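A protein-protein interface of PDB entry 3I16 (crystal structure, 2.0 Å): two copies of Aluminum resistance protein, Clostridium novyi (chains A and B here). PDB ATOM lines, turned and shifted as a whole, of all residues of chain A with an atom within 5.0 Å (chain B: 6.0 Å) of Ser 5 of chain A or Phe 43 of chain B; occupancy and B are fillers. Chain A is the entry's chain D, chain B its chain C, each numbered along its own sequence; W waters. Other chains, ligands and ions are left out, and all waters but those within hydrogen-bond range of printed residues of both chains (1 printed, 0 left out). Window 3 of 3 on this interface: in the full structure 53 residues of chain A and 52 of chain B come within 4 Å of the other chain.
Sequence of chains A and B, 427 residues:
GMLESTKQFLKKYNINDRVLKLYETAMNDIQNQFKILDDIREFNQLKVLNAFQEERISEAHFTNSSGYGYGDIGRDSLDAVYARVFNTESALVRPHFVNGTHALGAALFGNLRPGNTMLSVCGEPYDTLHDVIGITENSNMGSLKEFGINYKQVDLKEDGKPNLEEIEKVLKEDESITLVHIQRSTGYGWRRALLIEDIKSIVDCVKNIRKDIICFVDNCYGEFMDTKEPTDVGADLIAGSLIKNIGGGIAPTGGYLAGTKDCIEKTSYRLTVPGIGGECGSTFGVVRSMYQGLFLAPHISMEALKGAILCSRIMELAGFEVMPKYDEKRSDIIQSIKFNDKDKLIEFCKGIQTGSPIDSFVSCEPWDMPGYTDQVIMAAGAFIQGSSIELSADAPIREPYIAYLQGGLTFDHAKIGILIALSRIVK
Of the 7 printed residues of chain A, 4 touch a printed residue of chain B.
Hydrophobic or aromatic side chains of chain A that line the printed part of chain B: Leu 3 and Phe 9.
Of the 13 printed residues of chain B, 6 touch a printed residue of chain A.
Printed residues of chain B that touch a printed residue of chain A: Asp 39, Glu 42, Phe 43, Leu 46, Lys 47 and Thr 227.
Among the printed residues, 8 pairs touch across the chains.
Among the printed residues, no Asp or Glu carboxylate lies within 4 Å of a Lys or Arg side-chain nitrogen of the other chain.
Water W1 lies within hydrogen-bond range of OG1 of Thr 6 of chain A, O of Asp 39 of chain B, OE1 of Glu 42 of chain B and N of Leu 3 of chain A.
No position is printed for both chains.
Of the 8 pairs that touch across the chains among the printed residues, none has its exchanged pair printed and touching as well.
Ser 5 of chain A touches just one residue of chain B: Phe 43 (3.5 Å).
Phe 43 of chain B touches just these residues of chain A: Ser 5, Thr 6 and Phe 9.
Of the printed residues of chain B, Thr 6 of chain A touches Glu 42 (3.9 Å) and Phe 43 (3.4 Å).
Of the printed residues of chain A, Asp 39 of chain B touches Leu 3.
Of the printed residues of chain B, Leu 3 of chain A touches Asp 39 and Thr 227.
Of the printed residues of chain A, Thr 227 of chain B touches Leu 3 (3.6 Å).
The nearest printed residue of chain A that does not touch Asp 39 of chain B is Thr 6 of chain A (4.3 Å).
Leu 3 of chain A touches Asp 39 of chain B.
Leu 3 of chain A touches Thr 227 of chain B (CD1 to CG2, 3.6 Å).
Ser 5 of chain A touches Phe 43 of chain B (OG to CD1, 3.5 Å).
CG2 of Thr 6 of chain A touches OE1 of Glu 42 of chain B (3.9 Å).
OG1 of Thr 6 of chain A touches CB of Phe 43 of chain B, 3.4 Å away.
Phe 9 of chain A touches Phe 43 of chain B (CD2 to CE1, 3.7 Å).
Phe 9 of chain A touches Leu 46 of chain B (CG to CD2, 3.5 Å).
Phe 9 of chain A touches Lys 47 of chain B (CE2 to CA, 3.7 Å).
The side-chain amino group (NZ) of Lys 47 of chain B sits close to the side-chain amide oxygen (OD1) of Asn 44 of chain B (3.4 Å).
The side-chain amino group (NZ) of Lys 47 of chain B is in hydrogen-bond range of the backbone carbonyl oxygen (O) of Thr 227 of chain B, at 2.8 Å.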
ATOM      1  N   LEU A   3     -15.726  -4.903   2.534  1.00  0.00           N
ATOM      2  CA  LEU A   3     -16.077  -6.007   1.677  1.00  0.00           C
ATOM      3  C   LEU A   3     -17.582  -6.182   1.584  1.00  0.00           C
ATOM      4  O   LEU A   3     -18.323  -5.874   2.519  1.00  0.00           O
ATOM      5  CB  LEU A   3     -15.461  -7.318   2.184  1.00  0.00           C
ATOM      6  CG  LEU A   3     -13.955  -7.442   2.290  1.00  0.00           C
ATOM      7  CD1 LEU A   3     -13.596  -8.796   2.978  1.00  0.00           C
ATOM      8  CD2 LEU A   3     -13.353  -7.330   0.885  1.00  0.00           C
ATOM      9  N   GLU A   4     -18.032  -6.674   0.434  1.00  0.00           N
ATOM     10  CA  GLU A   4     -19.433  -6.963   0.243  1.00  0.00           C
ATOM     11  C   GLU A   4     -19.909  -7.990   1.266  1.00  0.00           C
ATOM     12  O   GLU A   4     -21.005  -7.875   1.793  1.00  0.00           O
ATOM     13  CB  GLU A   4     -19.670  -7.454  -1.186  1.00  0.00           C
ATOM     14  CG  GLU A   4     -21.107  -7.698  -1.517  1.00  0.00           C
ATOM     15  CD  GLU A   4     -21.955  -6.458  -1.352  1.00  0.00           C
ATOM     16  OE1 GLU A   4     -21.429  -5.320  -1.578  1.00  0.00           O
ATOM     17  OE2 GLU A   4     -23.144  -6.655  -1.003  1.00  0.00           O
ATOM     18  N   SER A   5     -19.075  -8.983   1.555  1.00  0.00           N
ATOM     19  CA  SER A   5     -19.384  -9.989   2.569  1.00  0.00           C
ATOM     20  C   SER A   5     -19.603  -9.339   3.969  1.00  0.00           C
ATOM     21  O   SER A   5     -20.517  -9.736   4.703  1.00  0.00           O
ATOM     22  CB  SER A   5     -18.266 -11.039   2.603  1.00  0.00           C
ATOM     23  OG  SER A   5     -17.014 -10.439   2.965  1.00  0.00           O
ATOM     24  N   THR A   6     -18.797  -8.334   4.307  1.00  0.00           N
ATOM     25  CA  THR A   6     -18.918  -7.620   5.564  1.00  0.00           C
ATOM     26  C   THR A   6     -20.223  -6.836   5.597  1.00  0.00           C
ATOM     27  O   THR A   6     -20.879  -6.769   6.650  1.00  0.00           O
ATOM     28  CB  THR A   6     -17.749  -6.623   5.809  1.00  0.00           C
ATOM     29  OG1 THR A   6     -16.490  -7.312   5.795  1.00  0.00           O
ATOM     30  CG2 THR A   6     -17.916  -5.898   7.148  1.00  0.00           C
ATOM     31  N   LYS A   7     -20.598  -6.238   4.455  1.00  0.00           N
ATOM     32  CA  LYS A   7     -21.856  -5.485   4.374  1.00  0.00           C
ATOM     33  C   LYS A   7     -23.018  -6.420   4.661  1.00  0.00           C
ATOM     34  O   LYS A   7     -23.903  -6.114   5.473  1.00  0.00           O
ATOM     35  CB  LYS A   7     -22.036  -4.790   3.012  1.00  0.00           C
ATOM     36  CG  LYS A   7     -20.982  -3.698   2.697  1.00  0.00           C
ATOM     37  CD  LYS A   7     -21.156  -3.037   1.307  1.00  0.00           C
ATOM     38  CE  LYS A   7     -19.952  -2.154   0.961  1.00  0.00           C
ATOM     39  NZ  LYS A   7     -20.101  -1.470  -0.347  1.00  0.00           N
ATOM     40  N   GLN A   8     -22.994  -7.592   4.051  1.00  0.00           N
ATOM     41  CA  GLN A   8     -24.051  -8.569   4.299  1.00  0.00           C
ATOM     42  C   GLN A   8     -24.068  -9.046   5.745  1.00  0.00           C
ATOM     43  O   GLN A   8     -25.121  -9.259   6.337  1.00  0.00           O
ATOM     44  CB  GLN A   8     -23.892  -9.766   3.364  1.00  0.00           C
ATOM     45  CG  GLN A   8     -24.111  -9.430   1.892  1.00  0.00           C
ATOM     46  CD  GLN A   8     -25.518  -8.944   1.623  1.00  0.00           C
ATOM     47  OE1 GLN A   8     -26.494  -9.510   2.142  1.00  0.00           O
ATOM     48  NE2 GLN A   8     -25.639  -7.880   0.814  1.00  0.00           N
ATOM     49  N   PHE A   9     -22.896  -9.177   6.329  1.00  0.00           N
ATOM     50  CA  PHE A   9     -22.794  -9.649   7.679  1.00  0.00           C
ATOM     51  C   PHE A   9     -23.375  -8.553   8.593  1.00  0.00           C
ATOM     52  O   PHE A   9     -24.104  -8.841   9.526  1.00  0.00           O
ATOM     53  CB  PHE A   9     -21.329  -9.901   8.016  1.00  0.00           C
ATOM     54  CG  PHE A   9     -21.091 -10.900   9.111  1.00  0.00           C
ATOM     55  CD1 PHE A   9     -22.043 -11.195  10.087  1.00  0.00           C
ATOM     56  CD2 PHE A   9     -19.838 -11.489   9.214  1.00  0.00           C
ATOM     57  CE1 PHE A   9     -21.776 -12.100  11.080  1.00  0.00           C
ATOM     58  CE2 PHE A   9     -19.552 -12.366  10.241  1.00  0.00           C
ATOM     59  CZ  PHE A   9     -20.532 -12.684  11.174  1.00  0.00           C
ATOM     60  N   ASP B  38      -6.849  -4.343   6.043  1.00  0.00           N
ATOM     61  CA  ASP B  38      -7.882  -3.774   6.921  1.00  0.00           C
ATOM     62  C   ASP B  38      -9.296  -4.272   6.600  1.00  0.00           C
ATOM     63  O   ASP B  38     -10.107  -4.434   7.510  1.00  0.00           O
ATOM     64  CB  ASP B  38      -7.846  -2.249   6.896  1.00  0.00           C
ATOM     65  CG  ASP B  38      -6.613  -1.690   7.549  1.00  0.00           C
ATOM     66  OD1 ASP B  38      -5.857  -2.480   8.174  1.00  0.00           O
ATOM     67  OD2 ASP B  38      -6.401  -0.455   7.424  1.00  0.00           O
ATOM     68  N   ASP B  39      -9.577  -4.524   5.320  1.00  0.00           N
ATOM     69  CA  ASP B  39     -10.875  -5.010   4.905  1.00  0.00           C
ATOM     70  C   ASP B  39     -11.109  -6.420   5.393  1.00  0.00           C
ATOM     71  O   ASP B  39     -12.213  -6.737   5.812  1.00  0.00           O
ATOM     72  CB  ASP B  39     -11.028  -4.951   3.399  1.00  0.00           C
ATOM     73  CG  ASP B  39     -10.962  -3.509   2.851  1.00  0.00           C
ATOM     74  OD1 ASP B  39     -11.230  -2.547   3.596  1.00  0.00           O
ATOM     75  OD2 ASP B  39     -10.628  -3.344   1.665  1.00  0.00           O
ATOM     76  N   ILE B  40     -10.075  -7.260   5.323  1.00  0.00           N
ATOM     77  CA  ILE B  40     -10.162  -8.644   5.777  1.00  0.00           C
ATOM     78  C   ILE B  40     -10.288  -8.650   7.320  1.00  0.00           C
ATOM     79  O   ILE B  40     -11.089  -9.379   7.875  1.00  0.00           O
ATOM     80  CB  ILE B  40      -8.908  -9.422   5.358  1.00  0.00           C
ATOM     81  CG1 ILE B  40      -8.848  -9.588   3.841  1.00  0.00           C
ATOM     82  CG2 ILE B  40      -8.835 -10.733   6.056  1.00  0.00           C
ATOM     83  CD1 ILE B  40      -7.449  -9.966   3.330  1.00  0.00           C
ATOM     84  N   ARG B  41      -9.489  -7.817   7.987  1.00  0.00           N
ATOM     85  CA  ARG B  41      -9.489  -7.751   9.453  1.00  0.00           C
ATOM     86  C   ARG B  41     -10.863  -7.361  10.014  1.00  0.00           C
ATOM     87  O   ARG B  41     -11.324  -7.911  11.010  1.00  0.00           O
ATOM     88  CB  ARG B  41      -8.455  -6.729   9.920  1.00  0.00           C
ATOM     89  CG  ARG B  41      -8.328  -6.566  11.425  1.00  0.00           C
ATOM     90  CD  ARG B  41      -7.380  -5.434  11.746  1.00  0.00           C
ATOM     91  NE  ARG B  41      -7.925  -4.146  11.318  1.00  0.00           N
ATOM     92  CZ  ARG B  41      -7.240  -2.998  11.282  1.00  0.00           C
ATOM     93  NH1 ARG B  41      -5.964  -2.942  11.639  1.00  0.00           N
ATOM     94  NH2 ARG B  41      -7.838  -1.890  10.856  1.00  0.00           N
ATOM     95  N   GLU B  42     -11.498  -6.396   9.362  1.00  0.00           N
ATOM     96  CA  GLU B  42     -12.820  -5.924   9.744  1.00  0.00           C
ATOM     97  C   GLU B  42     -13.803  -7.082   9.704  1.00  0.00           C
ATOM     98  O   GLU B  42     -14.525  -7.320  10.674  1.00  0.00           O
ATOM     99  CB  GLU B  42     -13.232  -4.796   8.803  1.00  0.00           C
ATOM    100  CG  GLU B  42     -14.575  -4.182   9.045  1.00  0.00           C
ATOM    101  CD  GLU B  42     -14.869  -3.099   8.022  1.00  0.00           C
ATOM    102  OE1 GLU B  42     -14.910  -3.402   6.799  1.00  0.00           O
ATOM    103  OE2 GLU B  42     -15.036  -1.942   8.449  1.00  0.00           O
ATOM    104  N   PHE B  43     -13.785  -7.838   8.616  1.00  0.00           N
ATOM    105  CA  PHE B  43     -14.644  -9.017   8.496  1.00  0.00           C
ATOM    106  C   PHE B  43     -14.385 -10.024   9.612  1.00  0.00           C
ATOM    107  O   PHE B  43     -15.334 -10.514  10.251  1.00  0.00           O
ATOM    108  CB  PHE B  43     -14.474  -9.729   7.155  1.00  0.00           C
ATOM    109  CG  PHE B  43     -15.409 -10.888   6.980  1.00  0.00           C
ATOM    110  CD1 PHE B  43     -16.696 -10.690   6.477  1.00  0.00           C
ATOM    111  CD2 PHE B  43     -15.032 -12.161   7.368  1.00  0.00           C
ATOM    112  CE1 PHE B  43     -17.584 -11.744   6.346  1.00  0.00           C
ATOM    113  CE2 PHE B  43     -15.908 -13.232   7.245  1.00  0.00           C
ATOM    114  CZ  PHE B  43     -17.190 -13.031   6.740  1.00  0.00           C
ATOM    115  N   ASN B  44     -13.114 -10.332   9.837  1.00  0.00           N
ATOM    116  CA  ASN B  44     -12.742 -11.336  10.849  1.00  0.00           C
ATOM    117  C   ASN B  44     -13.087 -10.926  12.289  1.00  0.00           C
ATOM    118  O   ASN B  44     -13.541 -11.752  13.098  1.00  0.00           O
ATOM    119  CB  ASN B  44     -11.271 -11.737  10.699  1.00  0.00           C
ATOM    120  CG  ASN B  44     -11.033 -12.580   9.480  1.00  0.00           C
ATOM    121  OD1 ASN B  44     -11.966 -13.188   8.943  1.00  0.00           O
ATOM    122  ND2 ASN B  44      -9.789 -12.638   9.030  1.00  0.00           N
ATOM    123  N   GLN B  45     -12.916  -9.642  12.593  1.00  0.00           N
ATOM    124  CA  GLN B  45     -13.300  -9.150  13.903  1.00  0.00           C
ATOM    125  C   GLN B  45     -14.800  -9.400  14.153  1.00  0.00           C
ATOM    126  O   GLN B  45     -15.209  -9.835  15.237  1.00  0.00           O
ATOM    127  CB  GLN B  45     -13.018  -7.657  14.020  1.00  0.00           C
ATOM    128  CG  GLN B  45     -13.354  -7.121  15.422  1.00  0.00           C
ATOM    129  CD  GLN B  45     -12.339  -7.565  16.447  1.00  0.00           C
ATOM    130  OE1 GLN B  45     -11.291  -6.948  16.562  1.00  0.00           O
ATOM    131  NE2 GLN B  45     -12.652  -8.618  17.214  1.00  0.00           N
ATOM    132  N   LEU B  46     -15.610  -9.090  13.146  1.00  0.00           N
ATOM    133  CA  LEU B  46     -17.046  -9.309  13.209  1.00  0.00           C
ATOM    134  C   LEU B  46     -17.373 -10.802  13.366  1.00  0.00           C
ATOM    135  O   LEU B  46     -18.254 -11.159  14.142  1.00  0.00           O
ATOM    136  CB  LEU B  46     -17.740  -8.702  11.974  1.00  0.00           C
ATOM    137  CG  LEU B  46     -19.280  -8.688  11.978  1.00  0.00           C
ATOM    138  CD1 LEU B  46     -19.839  -7.964  13.213  1.00  0.00           C
ATOM    139  CD2 LEU B  46     -19.784  -8.043  10.699  1.00  0.00           C
ATOM    140  N   LYS B  47     -16.679 -11.652  12.613  1.00  0.00           N
ATOM    141  CA  LYS B  47     -16.847 -13.109  12.675  1.00  0.00           C
ATOM    142  C   LYS B  47     -16.604 -13.621  14.104  1.00  0.00           C
ATOM    143  O   LYS B  47     -17.407 -14.401  14.657  1.00  0.00           O
ATOM    144  CB  LYS B  47     -15.899 -13.789  11.651  1.00  0.00           C
ATOM    145  CG  LYS B  47     -15.810 -15.310  11.754  1.00  0.00           C
ATOM    146  CD  LYS B  47     -15.106 -16.003  10.560  1.00  0.00           C
ATOM    147  CE  LYS B  47     -13.642 -15.688  10.403  1.00  0.00           C
ATOM    148  NZ  LYS B  47     -13.089 -16.341   9.163  1.00  0.00           N
ATOM    149  N   VAL B  48     -15.516 -13.189  14.701  1.00  0.00           N
ATOM    150  CA  VAL B  48     -15.217 -13.574  16.088  1.00  0.00           C
ATOM    151  C   VAL B  48     -16.239 -13.021  17.060  1.00  0.00           C
ATOM    152  O   VAL B  48     -16.747 -13.766  17.937  1.00  0.00           O
ATOM    153  CB  VAL B  48     -13.775 -13.200  16.529  1.00  0.00           C
ATOM    154  CG1 VAL B  48     -13.547 -13.595  18.022  1.00  0.00           C
ATOM    155  CG2 VAL B  48     -12.705 -13.894  15.603  1.00  0.00           C
ATOM    156  N   THR B 227     -10.577 -14.049   4.960  1.00  0.00           N
ATOM    157  CA  THR B 227     -11.904 -14.070   5.585  1.00  0.00           C
ATOM    158  C   THR B 227     -12.420 -15.511   5.713  1.00  0.00           C
ATOM    159  O   THR B 227     -13.383 -15.772   6.455  1.00  0.00           O
ATOM    160  CB  THR B 227     -12.902 -13.252   4.777  1.00  0.00           C
ATOM    161  OG1 THR B 227     -12.943 -13.800   3.467  1.00  0.00           O
ATOM    162  CG2 THR B 227     -12.476 -11.780   4.697  1.00  0.00           C
ATOM    163  N   LYS B 228     -11.813 -16.426   4.963  1.00  0.00           N
ATOM    164  CA  LYS B 228     -12.118 -17.849   5.034  1.00  0.00           C
ATOM    165  C   LYS B 228     -10.958 -18.618   5.656  1.00  0.00           C
ATOM    166  O   LYS B 228      -9.804 -18.193   5.562  1.00  0.00           O
ATOM    167  CB  LYS B 228     -12.376 -18.433   3.654  1.00  0.00           C
ATOM    168  CG  LYS B 228     -13.684 -18.047   3.051  1.00  0.00           C
ATOM    169  CD  LYS B 228     -13.954 -18.782   1.745  1.00  0.00           C
ATOM    170  CE  LYS B 228     -15.236 -18.256   1.076  1.00  0.00           C
ATOM    171  NZ  LYS B 228     -15.066 -16.859   0.585  1.00  0.00           N
HETATM  172  O   HOH W   1     -14.578  -5.602   5.230  1.00  0.00           O
